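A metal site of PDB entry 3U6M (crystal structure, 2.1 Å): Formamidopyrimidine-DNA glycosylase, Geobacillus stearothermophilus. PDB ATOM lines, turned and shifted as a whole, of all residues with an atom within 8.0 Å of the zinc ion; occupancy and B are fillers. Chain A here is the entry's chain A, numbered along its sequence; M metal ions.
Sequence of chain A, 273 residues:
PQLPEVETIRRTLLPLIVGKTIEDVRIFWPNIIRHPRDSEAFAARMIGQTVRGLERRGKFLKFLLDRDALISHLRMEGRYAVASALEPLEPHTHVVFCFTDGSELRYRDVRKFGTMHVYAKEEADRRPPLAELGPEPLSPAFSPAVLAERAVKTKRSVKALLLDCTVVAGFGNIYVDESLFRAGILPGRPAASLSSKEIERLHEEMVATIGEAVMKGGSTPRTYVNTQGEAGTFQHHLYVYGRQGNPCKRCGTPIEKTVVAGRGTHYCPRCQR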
ATOM      1  N   PHE A 181      12.865  -8.235   5.116  1.00  0.00           N
ATOM      2  CA  PHE A 181      11.841  -7.345   4.587  1.00  0.00           C
ATOM      3  C   PHE A 181      12.063  -7.142   3.083  1.00  0.00           C
ATOM      4  O   PHE A 181      11.131  -7.253   2.292  1.00  0.00           O
ATOM      5  CB  PHE A 181      11.832  -5.979   5.277  1.00  0.00           C
ATOM      6  CG  PHE A 181      10.977  -4.971   4.570  1.00  0.00           C
ATOM      7  CD1 PHE A 181       9.601  -4.955   4.760  1.00  0.00           C
ATOM      8  CD2 PHE A 181      11.534  -4.086   3.668  1.00  0.00           C
ATOM      9  CE1 PHE A 181       8.803  -4.032   4.083  1.00  0.00           C
ATOM     10  CE2 PHE A 181      10.744  -3.165   2.987  1.00  0.00           C
ATOM     11  CZ  PHE A 181       9.377  -3.148   3.196  1.00  0.00           C
ATOM     12  N   TYR A 239      13.849   0.047   6.799  1.00  0.00           N
ATOM     13  CA  TYR A 239      12.482  -0.225   6.397  1.00  0.00           C
ATOM     14  C   TYR A 239      11.639  -0.681   7.575  1.00  0.00           C
ATOM     15  O   TYR A 239      10.461  -0.310   7.689  1.00  0.00           O
ATOM     16  CB  TYR A 239      12.453  -1.274   5.299  1.00  0.00           C
ATOM     17  CG  TYR A 239      12.894  -0.731   3.963  1.00  0.00           C
ATOM     18  CD1 TYR A 239      14.114  -1.079   3.422  1.00  0.00           C
ATOM     19  CD2 TYR A 239      12.072   0.141   3.254  1.00  0.00           C
ATOM     20  CE1 TYR A 239      14.518  -0.584   2.192  1.00  0.00           C
ATOM     21  CE2 TYR A 239      12.468   0.647   2.028  1.00  0.00           C
ATOM     22  CZ  TYR A 239      13.694   0.280   1.506  1.00  0.00           C
ATOM     23  OH  TYR A 239      14.103   0.785   0.285  1.00  0.00           O
ATOM     24  N   VAL A 240      12.231  -1.494   8.443  1.00  0.00           N
ATOM     25  CA  VAL A 240      11.485  -2.121   9.525  1.00  0.00           C
ATOM     26  C   VAL A 240      12.136  -2.023  10.897  1.00  0.00           C
ATOM     27  O   VAL A 240      11.454  -1.846  11.899  1.00  0.00           O
ATOM     28  CB  VAL A 240      11.178  -3.591   9.224  1.00  0.00           C
ATOM     29  CG1 VAL A 240      10.326  -3.706   7.977  1.00  0.00           C
ATOM     30  CG2 VAL A 240      12.478  -4.395   9.062  1.00  0.00           C
ATOM     31  N   PRO A 247       4.114   3.329   9.895  1.00  0.00           N
ATOM     32  CA  PRO A 247       3.706   2.824   8.585  1.00  0.00           C
ATOM     33  C   PRO A 247       4.894   2.230   7.811  1.00  0.00           C
ATOM     34  O   PRO A 247       5.985   2.788   7.827  1.00  0.00           O
ATOM     35  CB  PRO A 247       3.199   4.071   7.856  1.00  0.00           C
ATOM     36  CG  PRO A 247       2.965   5.100   8.943  1.00  0.00           C
ATOM     37  CD  PRO A 247       3.978   4.798  10.003  1.00  0.00           C
ATOM     38  N   CYS A 248       4.666   1.097   7.158  1.00  0.00           N
ATOM     39  CA  CYS A 248       5.635   0.547   6.231  1.00  0.00           C
ATOM     40  C   CYS A 248       5.845   1.548   5.112  1.00  0.00           C
ATOM     41  O   CYS A 248       4.888   2.139   4.614  1.00  0.00           O
ATOM     42  CB  CYS A 248       5.135  -0.780   5.652  1.00  0.00           C
ATOM     43  SG  CYS A 248       6.164  -1.419   4.303  1.00  0.00           S
ATOM     44  N   LYS A 249       7.113   1.743   4.735  1.00  0.00           N
ATOM     45  CA  LYS A 249       7.484   2.733   3.730  1.00  0.00           C
ATOM     46  C   LYS A 249       7.100   2.289   2.331  1.00  0.00           C
ATOM     47  O   LYS A 249       7.087   3.098   1.395  1.00  0.00           O
ATOM     48  CB  LYS A 249       9.004   3.001   3.786  1.00  0.00           C
ATOM     49  CG  LYS A 249       9.485   3.560   5.116  1.00  0.00           C
ATOM     50  CD  LYS A 249      10.927   4.008   5.039  1.00  0.00           C
ATOM     51  CE  LYS A 249      11.374   4.592   6.384  1.00  0.00           C
ATOM     52  NZ  LYS A 249      12.765   5.140   6.329  1.00  0.00           N
ATOM     53  N   ARG A 250       6.778   1.013   2.176  1.00  0.00           N
ATOM     54  CA  ARG A 250       6.403   0.484   0.873  1.00  0.00           C
ATOM     55  C   ARG A 250       4.894   0.237   0.712  1.00  0.00           C
ATOM     56  O   ARG A 250       4.391   0.292  -0.412  1.00  0.00           O
ATOM     57  CB  ARG A 250       7.194  -0.776   0.549  1.00  0.00           C
ATOM     58  CG  ARG A 250       8.678  -0.525   0.336  1.00  0.00           C
ATOM     59  CD  ARG A 250       9.334  -1.650  -0.425  1.00  0.00           C
ATOM     60  NE  ARG A 250      10.670  -1.278  -0.881  1.00  0.00           N
ATOM     61  CZ  ARG A 250      11.608  -2.162  -1.204  1.00  0.00           C
ATOM     62  NH1 ARG A 250      11.355  -3.457  -1.105  1.00  0.00           N
ATOM     63  NH2 ARG A 250      12.794  -1.748  -1.614  1.00  0.00           N
ATOM     64  N   CYS A 251       4.186  -0.020   1.802  1.00  0.00           N
ATOM     65  CA  CYS A 251       2.745  -0.281   1.698  1.00  0.00           C
ATOM     66  C   CYS A 251       1.880   0.425   2.729  1.00  0.00           C
ATOM     67  O   CYS A 251       0.656   0.432   2.619  1.00  0.00           O
ATOM     68  CB  CYS A 251       2.478  -1.791   1.743  1.00  0.00           C
ATOM     69  SG  CYS A 251       2.512  -2.476   3.414  1.00  0.00           S
ATOM     70  N   GLY A 252       2.501   1.034   3.740  1.00  0.00           N
ATOM     71  CA  GLY A 252       1.765   1.851   4.699  1.00  0.00           C
ATOM     72  C   GLY A 252       1.171   1.091   5.868  1.00  0.00           C
ATOM     73  O   GLY A 252       0.619   1.702   6.790  1.00  0.00           O
ATOM     74  N   THR A 253       1.263  -0.225   5.831  1.00  0.00           N
ATOM     75  CA  THR A 253       0.784  -1.064   6.938  1.00  0.00           C
ATOM     76  C   THR A 253       1.677  -0.876   8.153  1.00  0.00           C
ATOM     77  O   THR A 253       2.896  -0.818   8.033  1.00  0.00           O
ATOM     78  CB  THR A 253       0.824  -2.534   6.522  1.00  0.00           C
ATOM     79  OG1 THR A 253      -0.024  -2.732   5.386  1.00  0.00           O
ATOM     80  CG2 THR A 253       0.371  -3.432   7.684  1.00  0.00           C
ATOM     81  N   PRO A 254       1.082  -0.775   9.348  1.00  0.00           N
ATOM     82  CA  PRO A 254       1.973  -0.551  10.497  1.00  0.00           C
ATOM     83  C   PRO A 254       2.995  -1.672  10.636  1.00  0.00           C
ATOM     84  O   PRO A 254       2.665  -2.855  10.504  1.00  0.00           O
ATOM     85  CB  PRO A 254       1.007  -0.548  11.689  1.00  0.00           C
ATOM     86  CG  PRO A 254      -0.333  -0.141  11.095  1.00  0.00           C
ATOM     87  CD  PRO A 254      -0.345  -0.787   9.750  1.00  0.00           C
ATOM     88  N   ILE A 255       4.239  -1.305  10.905  1.00  0.00           N
ATOM     89  CA  ILE A 255       5.267  -2.309  11.137  1.00  0.00           C
ATOM     90  C   ILE A 255       5.001  -2.984  12.462  1.00  0.00           C
ATOM     91  O   ILE A 255       4.614  -2.339  13.440  1.00  0.00           O
ATOM     92  CB  ILE A 255       6.678  -1.678  11.148  1.00  0.00           C
ATOM     93  CG1 ILE A 255       6.988  -1.113   9.761  1.00  0.00           C
ATOM     94  CG2 ILE A 255       7.731  -2.724  11.523  1.00  0.00           C
ATOM     95  CD1 ILE A 255       6.715  -2.106   8.620  1.00  0.00           C
ATOM     96  N   TYR A 267       8.958  -6.521  11.185  1.00  0.00           N
ATOM     97  CA  TYR A 267       8.538  -6.974   9.879  1.00  0.00           C
ATOM     98  C   TYR A 267       7.232  -6.283   9.484  1.00  0.00           C
ATOM     99  O   TYR A 267       6.484  -5.807  10.334  1.00  0.00           O
ATOM    100  CB  TYR A 267       8.326  -8.483   9.899  1.00  0.00           C
ATOM    101  CG  TYR A 267       7.218  -8.907  10.823  1.00  0.00           C
ATOM    102  CD1 TYR A 267       5.922  -9.091  10.354  1.00  0.00           C
ATOM    103  CD2 TYR A 267       7.444  -9.093  12.187  1.00  0.00           C
ATOM    104  CE1 TYR A 267       4.895  -9.461  11.196  1.00  0.00           C
ATOM    105  CE2 TYR A 267       6.429  -9.473  13.034  1.00  0.00           C
ATOM    106  CZ  TYR A 267       5.153  -9.652  12.534  1.00  0.00           C
ATOM    107  OH  TYR A 267       4.130 -10.021  13.385  1.00  0.00           O
ATOM    108  N   CYS A 268       6.979  -6.231   8.179  1.00  0.00           N
ATOM    109  CA  CYS A 268       5.692  -5.813   7.672  1.00  0.00           C
ATOM    110  C   CYS A 268       4.887  -7.047   7.319  1.00  0.00           C
ATOM    111  O   CYS A 268       5.301  -7.847   6.475  1.00  0.00           O
ATOM    112  CB  CYS A 268       5.858  -4.917   6.443  1.00  0.00           C
ATOM    113  SG  CYS A 268       4.253  -4.532   5.663  1.00  0.00           S
ATOM    114  N   PRO A 269       3.724  -7.213   7.966  1.00  0.00           N
ATOM    115  CA  PRO A 269       2.866  -8.389   7.768  1.00  0.00           C
ATOM    116  C   PRO A 269       2.224  -8.417   6.391  1.00  0.00           C
ATOM    117  O   PRO A 269       1.612  -9.420   6.044  1.00  0.00           O
ATOM    118  CB  PRO A 269       1.781  -8.209   8.834  1.00  0.00           C
ATOM    119  CG  PRO A 269       1.672  -6.731   8.973  1.00  0.00           C
ATOM    120  CD  PRO A 269       3.089  -6.213   8.841  1.00  0.00           C
ATOM    121  N   ARG A 270       2.343  -7.337   5.631  1.00  0.00           N
ATOM    122  CA  ARG A 270       1.819  -7.348   4.265  1.00  0.00           C
ATOM    123  C   ARG A 270       2.915  -7.618   3.229  1.00  0.00           C
ATOM    124  O   ARG A 270       2.742  -8.471   2.358  1.00  0.00           O
ATOM    125  CB  ARG A 270       1.077  -6.042   3.950  1.00  0.00           C
ATOM    126  CG  ARG A 270       0.455  -6.011   2.573  1.00  0.00           C
ATOM    127  CD  ARG A 270      -0.339  -4.714   2.316  1.00  0.00           C
ATOM    128  NE  ARG A 270      -0.919  -4.727   0.975  1.00  0.00           N
ATOM    129  CZ  ARG A 270      -1.738  -3.809   0.473  1.00  0.00           C
ATOM    130  NH1 ARG A 270      -2.201  -3.949  -0.764  1.00  0.00           N
ATOM    131  NH2 ARG A 270      -2.095  -2.751   1.208  1.00  0.00           N
ATOM    132  N   CYS A 271       4.027  -6.896   3.309  1.00  0.00           N
ATOM    133  CA  CYS A 271       5.113  -7.068   2.341  1.00  0.00           C
ATOM    134  C   CYS A 271       5.804  -8.400   2.504  1.00  0.00           C
ATOM    135  O   CYS A 271       6.321  -8.969   1.541  1.00  0.00           O
ATOM    136  CB  CYS A 271       6.154  -5.942   2.445  1.00  0.00           C
ATOM    137  SG  CYS A 271       5.543  -4.310   1.964  1.00  0.00           S
ATOM    138  N   GLN A 272       5.841  -8.908   3.730  1.00  0.00           N
ATOM    139  CA  GLN A 272       6.565 -10.158   3.964  1.00  0.00           C
ATOM    140  C   GLN A 272       5.595 -11.313   4.125  1.00  0.00           C
ATOM    141  O   GLN A 272       4.532 -11.152   4.708  1.00  0.00           O
ATOM    142  CB  GLN A 272       7.473 -10.032   5.184  1.00  0.00           C
ATOM    143  CG  GLN A 272       8.589  -9.030   4.959  1.00  0.00           C
ATOM    144  CD  GLN A 272       9.265  -8.630   6.236  1.00  0.00           C
ATOM    145  OE1 GLN A 272       9.043  -7.535   6.744  1.00  0.00           O
ATOM    146  NE2 GLN A 272      10.114  -9.519   6.768  1.00  0.00           N
HETATM  147 ZN    ZN M   1       4.748  -3.267   3.814  1.00  0.00          ZN
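SG of Cys 268 lies close to N of Arg 270 (3.4 Å).
N of Cys 268 is in hydrogen-bond range of OE1 of Gln 272, at 2.8 Å.
The side-chain sulfur (SG) of Cys 248 lies close to the backbone NH (N) of Arg 250, 3.3 Å away.
The backbone NH (N) of Cys 248 lies within hydrogen-bond range of the backbone carbonyl oxygen (O) of Thr 253 (2.8 Å).
The side-chain hydroxyl (OG1) of Thr 253 lies close to the side-chain sulfur (SG) of Cys 251 (3.2 Å).
Of the 18 residues printed, 4 come within 4 Å of the zinc ion.
The side-chain sulfur (SG) of Cys 271 is bound to the zinc ion, 2.3 Å away.
SG of Cys 268 is bound to the zinc ion (2.3 Å).
The zinc ion is bound by the side-chain sulfur (SG) of Cys 248, at 2.4 Å.
The side-chain sulfur (SG) of Cys 251 binds the zinc ion, at 2.4 Å.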
